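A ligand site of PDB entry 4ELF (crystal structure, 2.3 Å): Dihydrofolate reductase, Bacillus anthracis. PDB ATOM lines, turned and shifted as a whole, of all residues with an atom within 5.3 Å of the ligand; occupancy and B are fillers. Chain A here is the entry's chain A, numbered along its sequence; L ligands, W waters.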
ATOM      1  N   MET A   6     -29.565 -10.225  22.949  1.00  0.00           N
ATOM      2  CA  MET A   6     -28.629 -11.158  22.316  1.00  0.00           C
ATOM      3  C   MET A   6     -27.201 -10.762  22.716  1.00  0.00           C
ATOM      4  O   MET A   6     -26.740  -9.653  22.414  1.00  0.00           O
ATOM      5  CB  MET A   6     -28.788 -11.136  20.793  1.00  0.00           C
ATOM      6  CG  MET A   6     -27.683 -11.839  20.024  1.00  0.00           C
ATOM      7  SD  MET A   6     -27.565 -13.615  20.364  1.00  0.00           S
ATOM      8  CE  MET A   6     -29.100 -14.220  19.622  1.00  0.00           C
ATOM      9  N   VAL A   7     -26.523 -11.638  23.441  1.00  0.00           N
ATOM     10  CA  VAL A   7     -25.228 -11.268  24.028  1.00  0.00           C
ATOM     11  C   VAL A   7     -24.218 -12.435  24.138  1.00  0.00           C
ATOM     12  O   VAL A   7     -24.583 -13.608  24.395  1.00  0.00           O
ATOM     13  CB  VAL A   7     -25.412 -10.535  25.395  1.00  0.00           C
ATOM     14  CG1 VAL A   7     -26.007 -11.451  26.440  1.00  0.00           C
ATOM     15  CG2 VAL A   7     -24.097  -9.950  25.896  1.00  0.00           C
ATOM     16  N   ALA A   8     -22.945 -12.104  23.922  1.00  0.00           N
ATOM     17  CA  ALA A   8     -21.848 -13.035  24.157  1.00  0.00           C
ATOM     18  C   ALA A   8     -20.906 -12.394  25.144  1.00  0.00           C
ATOM     19  O   ALA A   8     -20.459 -11.270  24.919  1.00  0.00           O
ATOM     20  CB  ALA A   8     -21.105 -13.340  22.860  1.00  0.00           C
ATOM     21  N   ILE A  15     -17.909  -7.735  27.308  1.00  0.00           N
ATOM     22  CA  ILE A  15     -18.468  -7.874  25.971  1.00  0.00           C
ATOM     23  C   ILE A  15     -17.627  -7.177  24.901  1.00  0.00           C
ATOM     24  O   ILE A  15     -17.927  -7.281  23.713  1.00  0.00           O
ATOM     25  CB  ILE A  15     -19.925  -7.430  25.891  1.00  0.00           C
ATOM     26  CG1 ILE A  15     -20.067  -5.928  26.172  1.00  0.00           C
ATOM     27  CG2 ILE A  15     -20.776  -8.263  26.850  1.00  0.00           C
ATOM     28  CD1 ILE A  15     -21.505  -5.419  26.069  1.00  0.00           C
ATOM     29  N   ASN A  19     -13.797  -1.445  21.564  1.00  0.00           N
ATOM     30  CA  ASN A  19     -14.793  -1.608  20.506  1.00  0.00           C
ATOM     31  C   ASN A  19     -14.465  -2.786  19.594  1.00  0.00           C
ATOM     32  O   ASN A  19     -14.286  -2.627  18.385  1.00  0.00           O
ATOM     33  CB  ASN A  19     -14.924  -0.301  19.703  1.00  0.00           C
ATOM     34  CG  ASN A  19     -15.308   0.872  20.569  1.00  0.00           C
ATOM     35  OD1 ASN A  19     -16.202   0.761  21.431  1.00  0.00           O
ATOM     36  ND2 ASN A  19     -14.643   2.012  20.370  1.00  0.00           N
ATOM     37  N   ASN A  20     -14.382  -3.952  20.200  1.00  0.00           N
ATOM     38  CA  ASN A  20     -14.027  -5.162  19.495  1.00  0.00           C
ATOM     39  C   ASN A  20     -14.364  -6.373  20.348  1.00  0.00           C
ATOM     40  O   ASN A  20     -14.407  -6.281  21.577  1.00  0.00           O
ATOM     41  CB  ASN A  20     -12.542  -5.170  19.155  1.00  0.00           C
ATOM     42  CG  ASN A  20     -12.254  -4.644  17.759  1.00  0.00           C
ATOM     43  OD1 ASN A  20     -12.529  -5.317  16.762  1.00  0.00           O
ATOM     44  ND2 ASN A  20     -11.689  -3.428  17.689  1.00  0.00           N
ATOM     45  N   LEU A  21     -14.612  -7.512  19.707  1.00  0.00           N
ATOM     46  CA  LEU A  21     -14.700  -8.758  20.441  1.00  0.00           C
ATOM     47  C   LEU A  21     -13.278  -9.231  20.755  1.00  0.00           C
ATOM     48  O   LEU A  21     -12.398  -9.209  19.889  1.00  0.00           O
ATOM     49  CB  LEU A  21     -15.435  -9.814  19.623  1.00  0.00           C
ATOM     50  CG  LEU A  21     -16.922  -9.617  19.393  1.00  0.00           C
ATOM     51  CD1 LEU A  21     -17.457 -10.848  18.691  1.00  0.00           C
ATOM     52  CD2 LEU A  21     -17.659  -9.375  20.716  1.00  0.00           C
ATOM     53  N   PRO A  26     -16.133 -18.070  15.078  1.00  0.00           N
ATOM     54  CA  PRO A  26     -17.072 -17.973  13.942  1.00  0.00           C
ATOM     55  C   PRO A  26     -18.357 -18.768  14.191  1.00  0.00           C
ATOM     56  O   PRO A  26     -19.438 -18.292  13.784  1.00  0.00           O
ATOM     57  CB  PRO A  26     -16.304 -18.614  12.773  1.00  0.00           C
ATOM     58  CG  PRO A  26     -14.860 -18.625  13.203  1.00  0.00           C
ATOM     59  CD  PRO A  26     -14.819 -18.644  14.685  1.00  0.00           C
ATOM     60  N   GLU A  28     -19.926 -19.278  16.975  1.00  0.00           N
ATOM     61  CA  GLU A  28     -20.819 -18.417  17.766  1.00  0.00           C
ATOM     62  C   GLU A  28     -21.578 -17.447  16.867  1.00  0.00           C
ATOM     63  O   GLU A  28     -22.803 -17.360  16.922  1.00  0.00           O
ATOM     64  CB  GLU A  28     -20.055 -17.643  18.846  1.00  0.00           C
ATOM     65  CG  GLU A  28     -20.869 -17.378  20.111  1.00  0.00           C
ATOM     66  CD  GLU A  28     -21.776 -16.144  19.995  1.00  0.00           C
ATOM     67  OE1 GLU A  28     -21.313 -15.153  19.379  1.00  0.00           O
ATOM     68  OE2 GLU A  28     -22.910 -16.158  20.536  1.00  0.00           O
ATOM     69  N   LEU A  29     -20.854 -16.717  16.028  1.00  0.00           N
ATOM     70  CA  LEU A  29     -21.502 -15.775  15.125  1.00  0.00           C
ATOM     71  C   LEU A  29     -22.496 -16.465  14.189  1.00  0.00           C
ATOM     72  O   LEU A  29     -23.496 -15.860  13.786  1.00  0.00           O
ATOM     73  CB  LEU A  29     -20.463 -14.965  14.352  1.00  0.00           C
ATOM     74  CG  LEU A  29     -19.521 -14.256  15.332  1.00  0.00           C
ATOM     75  CD1 LEU A  29     -18.479 -13.391  14.608  1.00  0.00           C
ATOM     76  CD2 LEU A  29     -20.325 -13.425  16.353  1.00  0.00           C
ATOM     77  N   GLN A  30     -22.245 -17.723  13.851  1.00  0.00           N
ATOM     78  CA  GLN A  30     -23.211 -18.428  12.997  1.00  0.00           C
ATOM     79  C   GLN A  30     -24.475 -18.805  13.795  1.00  0.00           C
ATOM     80  O   GLN A  30     -25.573 -18.856  13.234  1.00  0.00           O
ATOM     81  CB  GLN A  30     -22.601 -19.666  12.340  1.00  0.00           C
ATOM     82  CG  GLN A  30     -23.582 -20.380  11.417  1.00  0.00           C
ATOM     83  CD  GLN A  30     -23.857 -19.609  10.124  1.00  0.00           C
ATOM     84  OE1 GLN A  30     -23.022 -18.824   9.657  1.00  0.00           O
ATOM     85  NE2 GLN A  30     -25.028 -19.852   9.529  1.00  0.00           N
ATOM     86  N   VAL A  32     -25.656 -16.811  16.264  1.00  0.00           N
ATOM     87  CA  VAL A  32     -26.333 -15.511  16.223  1.00  0.00           C
ATOM     88  C   VAL A  32     -27.086 -15.358  14.919  1.00  0.00           C
ATOM     89  O   VAL A  32     -28.262 -14.989  14.914  1.00  0.00           O
ATOM     90  CB  VAL A  32     -25.348 -14.339  16.350  1.00  0.00           C
ATOM     91  CG1 VAL A  32     -26.100 -13.004  16.224  1.00  0.00           C
ATOM     92  CG2 VAL A  32     -24.594 -14.406  17.663  1.00  0.00           C
ATOM     93  N   LYS A  33     -26.412 -15.651  13.801  1.00  0.00           N
ATOM     94  CA  LYS A  33     -27.038 -15.475  12.496  1.00  0.00           C
ATOM     95  C   LYS A  33     -28.292 -16.329  12.352  1.00  0.00           C
ATOM     96  O   LYS A  33     -29.337 -15.845  11.920  1.00  0.00           O
ATOM     97  CB  LYS A  33     -26.080 -15.761  11.345  1.00  0.00           C
ATOM     98  CG  LYS A  33     -26.766 -15.678   9.975  1.00  0.00           C
ATOM     99  CD  LYS A  33     -25.830 -16.070   8.827  1.00  0.00           C
ATOM    100  CE  LYS A  33     -26.601 -16.162   7.509  1.00  0.00           C
ATOM    101  NZ  LYS A  33     -25.678 -16.300   6.360  1.00  0.00           N
ATOM    102  N   THR A  36     -31.273 -14.990  14.886  1.00  0.00           N
ATOM    103  CA  THR A  36     -31.885 -13.665  14.666  1.00  0.00           C
ATOM    104  C   THR A  36     -32.490 -13.504  13.261  1.00  0.00           C
ATOM    105  O   THR A  36     -32.996 -12.419  12.924  1.00  0.00           O
ATOM    106  CB  THR A  36     -30.858 -12.525  14.876  1.00  0.00           C
ATOM    107  OG1 THR A  36     -29.726 -12.739  14.009  1.00  0.00           O
ATOM    108  CG2 THR A  36     -30.378 -12.475  16.305  1.00  0.00           C
ATOM    109  N   LEU A  41     -32.200  -6.483  14.304  1.00  0.00           N
ATOM    110  CA  LEU A  41     -31.068  -6.341  15.208  1.00  0.00           C
ATOM    111  C   LEU A  41     -31.006  -4.911  15.717  1.00  0.00           C
ATOM    112  O   LEU A  41     -30.949  -3.984  14.918  1.00  0.00           O
ATOM    113  CB  LEU A  41     -29.754  -6.619  14.476  1.00  0.00           C
ATOM    114  CG  LEU A  41     -29.538  -8.073  14.138  1.00  0.00           C
ATOM    115  CD1 LEU A  41     -28.175  -8.238  13.479  1.00  0.00           C
ATOM    116  CD2 LEU A  41     -29.648  -8.879  15.427  1.00  0.00           C
ATOM    117  N   ASN A  47     -21.401  -0.056  18.615  1.00  0.00           N
ATOM    118  CA  ASN A  47     -21.514  -1.487  18.360  1.00  0.00           C
ATOM    119  C   ASN A  47     -21.501  -1.659  16.848  1.00  0.00           C
ATOM    120  O   ASN A  47     -20.716  -2.461  16.332  1.00  0.00           O
ATOM    121  CB  ASN A  47     -22.781  -2.060  18.996  1.00  0.00           C
ATOM    122  CG  ASN A  47     -22.694  -3.569  19.262  1.00  0.00           C
ATOM    123  OD1 ASN A  47     -23.517  -4.346  18.762  1.00  0.00           O
ATOM    124  ND2 ASN A  47     -21.704  -3.980  20.036  1.00  0.00           N
ATOM    125  N   ALA A  50     -18.122  -1.094  15.208  1.00  0.00           N
ATOM    126  CA  ALA A  50     -17.187  -2.147  15.622  1.00  0.00           C
ATOM    127  C   ALA A  50     -17.437  -3.408  14.800  1.00  0.00           C
ATOM    128  O   ALA A  50     -16.505  -4.173  14.511  1.00  0.00           O
ATOM    129  CB  ALA A  50     -17.334  -2.438  17.117  1.00  0.00           C
ATOM    130  N   ILE A  51     -18.700  -3.610  14.427  1.00  0.00           N
ATOM    131  CA  ILE A  51     -19.101  -4.711  13.564  1.00  0.00           C
ATOM    132  C   ILE A  51     -18.667  -4.453  12.110  1.00  0.00           C
ATOM    133  O   ILE A  51     -18.220  -5.362  11.413  1.00  0.00           O
ATOM    134  CB  ILE A  51     -20.627  -4.937  13.633  1.00  0.00           C
ATOM    135  CG1 ILE A  51     -21.014  -5.494  15.014  1.00  0.00           C
ATOM    136  CG2 ILE A  51     -21.095  -5.848  12.501  1.00  0.00           C
ATOM    137  CD1 ILE A  51     -22.492  -5.341  15.344  1.00  0.00           C
ATOM    138  N   ARG A  53     -20.319  -3.185   9.186  1.00  0.00           N
ATOM    139  CA  ARG A  53     -21.181  -3.184   7.989  1.00  0.00           C
ATOM    140  C   ARG A  53     -22.577  -3.711   8.307  1.00  0.00           C
ATOM    141  O   ARG A  53     -22.772  -4.402   9.321  1.00  0.00           O
ATOM    142  CB  ARG A  53     -20.546  -3.997   6.853  1.00  0.00           C
ATOM    143  CG  ARG A  53     -20.783  -5.514   6.906  1.00  0.00           C
ATOM    144  CD  ARG A  53     -20.008  -6.176   8.029  1.00  0.00           C
ATOM    145  NE  ARG A  53     -20.167  -7.636   8.022  1.00  0.00           N
ATOM    146  CZ  ARG A  53     -19.675  -8.449   8.947  1.00  0.00           C
ATOM    147  NH1 ARG A  53     -18.991  -7.963   9.980  1.00  0.00           N
ATOM    148  NH2 ARG A  53     -19.871  -9.761   8.857  1.00  0.00           N
ATOM    149  N   LEU A  55     -25.447  -6.128   8.603  1.00  0.00           N
ATOM    150  CA  LEU A  55     -25.521  -7.580   8.599  1.00  0.00           C
ATOM    151  C   LEU A  55     -26.750  -8.016   7.784  1.00  0.00           C
ATOM    152  O   LEU A  55     -27.885  -7.702   8.149  1.00  0.00           O
ATOM    153  CB  LEU A  55     -25.580  -8.116  10.027  1.00  0.00           C
ATOM    154  CG  LEU A  55     -24.351  -7.824  10.893  1.00  0.00           C
ATOM    155  CD1 LEU A  55     -24.525  -8.358  12.311  1.00  0.00           C
ATOM    156  CD2 LEU A  55     -23.131  -8.434  10.248  1.00  0.00           C
ATOM    157  N   PRO A  56     -26.504  -8.731   6.673  1.00  0.00           N
ATOM    158  CA  PRO A  56     -27.531  -9.078   5.675  1.00  0.00           C
ATOM    159  C   PRO A  56     -28.625  -9.997   6.181  1.00  0.00           C
ATOM    160  O   PRO A  56     -28.446 -10.673   7.196  1.00  0.00           O
ATOM    161  CB  PRO A  56     -26.739  -9.775   4.567  1.00  0.00           C
ATOM    162  CG  PRO A  56     -25.463 -10.210   5.207  1.00  0.00           C
ATOM    163  CD  PRO A  56     -25.158  -9.169   6.245  1.00  0.00           C
ATOM    164  N   ARG A  58     -31.372  -9.084   7.432  1.00  0.00           N
ATOM    165  CA  ARG A  58     -31.672  -8.581   8.767  1.00  0.00           C
ATOM    166  C   ARG A  58     -31.980  -7.094   8.768  1.00  0.00           C
ATOM    167  O   ARG A  58     -31.276  -6.291   8.142  1.00  0.00           O
ATOM    168  CB  ARG A  58     -30.462  -8.831   9.668  1.00  0.00           C
ATOM    169  CG  ARG A  58     -30.739  -9.619  10.928  1.00  0.00           C
ATOM    170  CD  ARG A  58     -29.839 -10.826  10.985  1.00  0.00           C
ATOM    171  NE  ARG A  58     -30.078 -11.692   9.846  1.00  0.00           N
ATOM    172  CZ  ARG A  58     -30.185 -13.018   9.938  1.00  0.00           C
ATOM    173  NH1 ARG A  58     -30.035 -13.586  11.127  1.00  0.00           N
ATOM    174  NH2 ARG A  58     -30.415 -13.757   8.859  1.00  0.00           N
ATOM    175  N   ILE A  95     -31.914  -7.069  20.845  1.00  0.00           N
ATOM    176  CA  ILE A  95     -31.035  -6.025  21.310  1.00  0.00           C
ATOM    177  C   ILE A  95     -29.622  -6.611  21.226  1.00  0.00           C
ATOM    178  O   ILE A  95     -29.317  -7.646  21.858  1.00  0.00           O
ATOM    179  CB  ILE A  95     -31.436  -5.602  22.708  1.00  0.00           C
ATOM    180  CG1 ILE A  95     -32.950  -5.347  22.762  1.00  0.00           C
ATOM    181  CG2 ILE A  95     -30.635  -4.394  23.141  1.00  0.00           C
ATOM    182  CD1 ILE A  95     -33.461  -4.368  21.732  1.00  0.00           C
ATOM    183  N   PHE A  96     -28.787  -5.963  20.429  1.00  0.00           N
ATOM    184  CA  PHE A  96     -27.554  -6.552  19.936  1.00  0.00           C
ATOM    185  C   PHE A  96     -26.350  -5.954  20.629  1.00  0.00           C
ATOM    186  O   PHE A  96     -25.194  -6.377  20.395  1.00  0.00           O
ATOM    187  CB  PHE A  96     -27.453  -6.348  18.436  1.00  0.00           C
ATOM    188  CG  PHE A  96     -26.630  -7.392  17.748  1.00  0.00           C
ATOM    189  CD1 PHE A  96     -26.800  -8.729  18.056  1.00  0.00           C
ATOM    190  CD2 PHE A  96     -25.709  -7.047  16.771  1.00  0.00           C
ATOM    191  CE1 PHE A  96     -26.059  -9.710  17.430  1.00  0.00           C
ATOM    192  CE2 PHE A  96     -24.954  -8.039  16.133  1.00  0.00           C
ATOM    193  CZ  PHE A  96     -25.148  -9.366  16.467  1.00  0.00           C
ATOM    194  N   GLY A  97     -26.603  -4.959  21.471  1.00  0.00           N
ATOM    195  CA  GLY A  97     -25.551  -4.503  22.335  1.00  0.00           C
ATOM    196  C   GLY A  97     -25.092  -3.086  22.145  1.00  0.00           C
ATOM    197  O   GLY A  97     -25.692  -2.292  21.397  1.00  0.00           O
ATOM    198  N   TYR A 102     -28.344  -2.135  26.086  1.00  0.00           N
ATOM    199  CA  TYR A 102     -28.979  -3.117  26.956  1.00  0.00           C
ATOM    200  C   TYR A 102     -29.684  -2.396  28.106  1.00  0.00           C
ATOM    201  O   TYR A 102     -30.835  -2.697  28.418  1.00  0.00           O
ATOM    202  CB  TYR A 102     -27.954  -4.095  27.539  1.00  0.00           C
ATOM    203  CG  TYR A 102     -27.318  -5.003  26.515  1.00  0.00           C
ATOM    204  CD1 TYR A 102     -28.097  -5.763  25.651  1.00  0.00           C
ATOM    205  CD2 TYR A 102     -25.933  -5.100  26.414  1.00  0.00           C
ATOM    206  CE1 TYR A 102     -27.522  -6.596  24.711  1.00  0.00           C
ATOM    207  CE2 TYR A 102     -25.344  -5.933  25.491  1.00  0.00           C
ATOM    208  CZ  TYR A 102     -26.138  -6.681  24.639  1.00  0.00           C
ATOM    209  OH  TYR A 102     -25.564  -7.499  23.706  1.00  0.00           O
ATOM    210  N   THR A 115     -24.609 -16.079  25.368  1.00  0.00           N
ATOM    211  CA  THR A 115     -23.531 -17.049  25.177  1.00  0.00           C
ATOM    212  C   THR A 115     -22.490 -16.772  26.277  1.00  0.00           C
ATOM    213  O   THR A 115     -22.000 -15.635  26.359  1.00  0.00           O
ATOM    214  CB  THR A 115     -22.845 -16.917  23.789  1.00  0.00           C
ATOM    215  OG1 THR A 115     -23.811 -17.072  22.752  1.00  0.00           O
ATOM    216  CG2 THR A 115     -21.784 -17.966  23.614  1.00  0.00           C
HETATM  217  O1  LIG L   1     -20.494 -10.927  11.803  1.00  0.00           O
HETATM  218  C1  LIG L   1     -21.404 -11.087  12.586  1.00  0.00           C
HETATM  219  N1  LIG L   1     -22.580 -11.786  12.193  1.00  0.00           N
HETATM  220  N2  LIG L   1     -23.584 -11.944  13.101  1.00  0.00           N
HETATM  221  C2  LIG L   1     -24.879 -12.275  12.666  1.00  0.00           C
HETATM  222  C3  LIG L   1     -25.166 -12.234  11.219  1.00  0.00           C
HETATM  223  C4  LIG L   1     -26.524 -12.158  10.756  1.00  0.00           C
HETATM  224  C5  LIG L   1     -26.772 -12.111   9.393  1.00  0.00           C
HETATM  225  C6  LIG L   1     -25.726 -12.157   8.495  1.00  0.00           C
HETATM  226  C7  LIG L   1     -24.387 -12.226   8.951  1.00  0.00           C
HETATM  227  C8  LIG L   1     -24.144 -12.268  10.347  1.00  0.00           C
HETATM  228  C9  LIG L   1     -22.725 -12.352  10.858  1.00  0.00           C
HETATM  229  C10 LIG L   1     -22.341 -13.831  10.876  1.00  0.00           C
HETATM  230  C11 LIG L   1     -21.868 -14.470   9.579  1.00  0.00           C
HETATM  231  C12 LIG L   1     -20.880 -15.617   9.625  1.00  0.00           C
HETATM  232  F1  LIG L   1     -21.590 -16.748   9.511  1.00  0.00           F
HETATM  233  F2  LIG L   1     -20.174 -15.639  10.767  1.00  0.00           F
HETATM  234  F3  LIG L   1     -20.029 -15.474   8.594  1.00  0.00           F
HETATM  235  C13 LIG L   1     -21.350 -10.547  14.010  1.00  0.00           C
HETATM  236  C14 LIG L   1     -20.287  -9.742  14.419  1.00  0.00           C
HETATM  237  C15 LIG L   1     -20.230  -9.055  15.802  1.00  0.00           C
HETATM  238  C16 LIG L   1     -19.138  -8.267  16.088  1.00  0.00           C
HETATM  239  O2  LIG L   1     -18.093  -8.134  15.164  1.00  0.00           O
HETATM  240  C17 LIG L   1     -17.038  -9.067  15.207  1.00  0.00           C
HETATM  241  C18 LIG L   1     -19.032  -7.617  17.326  1.00  0.00           C
HETATM  242  O3  LIG L   1     -17.925  -6.840  17.600  1.00  0.00           O
HETATM  243  C19 LIG L   1     -17.931  -6.016  18.705  1.00  0.00           C
HETATM  244  C20 LIG L   1     -20.055  -7.760  18.279  1.00  0.00           C
HETATM  245  C21 LIG L   1     -21.163  -8.542  18.017  1.00  0.00           C
HETATM  246  C22 LIG L   1     -22.265  -8.643  19.123  1.00  0.00           C
HETATM  247  C23 LIG L   1     -22.672 -10.054  19.555  1.00  0.00           C
HETATM  248  C24 LIG L   1     -21.968 -11.195  19.157  1.00  0.00           C
HETATM  249  N3  LIG L   1     -22.399 -12.411  19.575  1.00  0.00           N
HETATM  250  C25 LIG L   1     -23.487 -12.548  20.384  1.00  0.00           C
HETATM  251  N4  LIG L   1     -23.906 -13.846  20.790  1.00  0.00           N
HETATM  252  N5  LIG L   1     -24.190 -11.469  20.778  1.00  0.00           N
HETATM  253  C26 LIG L   1     -23.804 -10.223  20.408  1.00  0.00           C
HETATM  254  N6  LIG L   1     -24.550  -9.091  20.854  1.00  0.00           N
HETATM  255  C27 LIG L   1     -21.262  -9.194  16.756  1.00  0.00           C
HETATM  256  O   HOH W   1     -17.353 -15.102  11.053  1.00  0.00           O
HETATM  257  O   HOH W   2     -19.213 -18.896  10.209  1.00  0.00           O
HETATM  258  O   HOH W   3     -15.499  -6.069  15.674  1.00  0.00           O
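The backbone carbonyl oxygen of Lys 33 is in hydrogen-bond range of the guanidinium group of Arg 58 (2.5 Å).
The side-chain amide oxygen (OD1) of Asn 47 sits close to the backbone carbonyl oxygen (O) of Phe 96, at 3.1 Å.
NH1 of Arg 53 is in hydrogen-bond range of O of Ile 51, 3.1 Å away.
NH1 of Arg 58 is in hydrogen-bond range of OG1 of Thr 36 (3.0 Å).
The backbone NH (N) of Met 6 sits at hydrogen-bond distance from the backbone carbonyl oxygen (O) of Ile 95.
OG1 of Thr 36 lies within hydrogen-bond range of O of Val 32, at 2.8 Å.
The side-chain carboxylate (OE2) of Glu 28 sits at hydrogen-bond distance from the side-chain hydroxyl (OG1) of Thr 115 (2.6 Å).
O of Pro 56 is in hydrogen-bond range of NE of Arg 58, at 3.3 Å.
F1 of the ligand sits close to OE1 of Gln 30, 2.5 Å away.
Residues that only touch the ligand: Pro 56 (3.1 Å), Val 32 (3.3 Å), Arg 58 (3.4 Å), Val 7 (3.4 Å), Leu 21 (3.5 Å), Ile 51 (3.5 Å), Lys 33 (3.6 Å), Leu 29 (3.7 Å), Thr 115 (3.8 Å), Leu 55 (3.8 Å), Asn 20 (3.9 Å) and Ala 50 (3.96 Å).
Hydrophobic or aromatic side chains within 4 Å of the ligand: Met 6, Ala 8, Leu 21, Leu 29, Val 32, Ala 50, Ile 51, Leu 55, Pro 56 and Phe 96.
Of the 27 residues printed, 19 come within 4 Å of the ligand.
N4 of the ligand lies within hydrogen-bond range of OE2 of Glu 28 (2.5 Å).
The backbone NH of Ala 8 lies within hydrogen-bond range of a nitrogen (N5) of the ligand.
SD of Met 6 sits at hydrogen-bond distance from N4 of the ligand (3.7 Å).
OH of Tyr 102 lies within hydrogen-bond range of N6 of the ligand, at 3.4 Å.
A nitrogen (N6) of the ligand sits at hydrogen-bond distance from the backbone carbonyl oxygen of Phe 96, 2.8 Å away.
A nitrogen (N6) of the ligand is in hydrogen-bond range of the backbone carbonyl oxygen (O) of Met 6 (2.7 Å).
NH2 of Arg 53 sits at hydrogen-bond distance from O1 of the ligand (3.2 Å).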
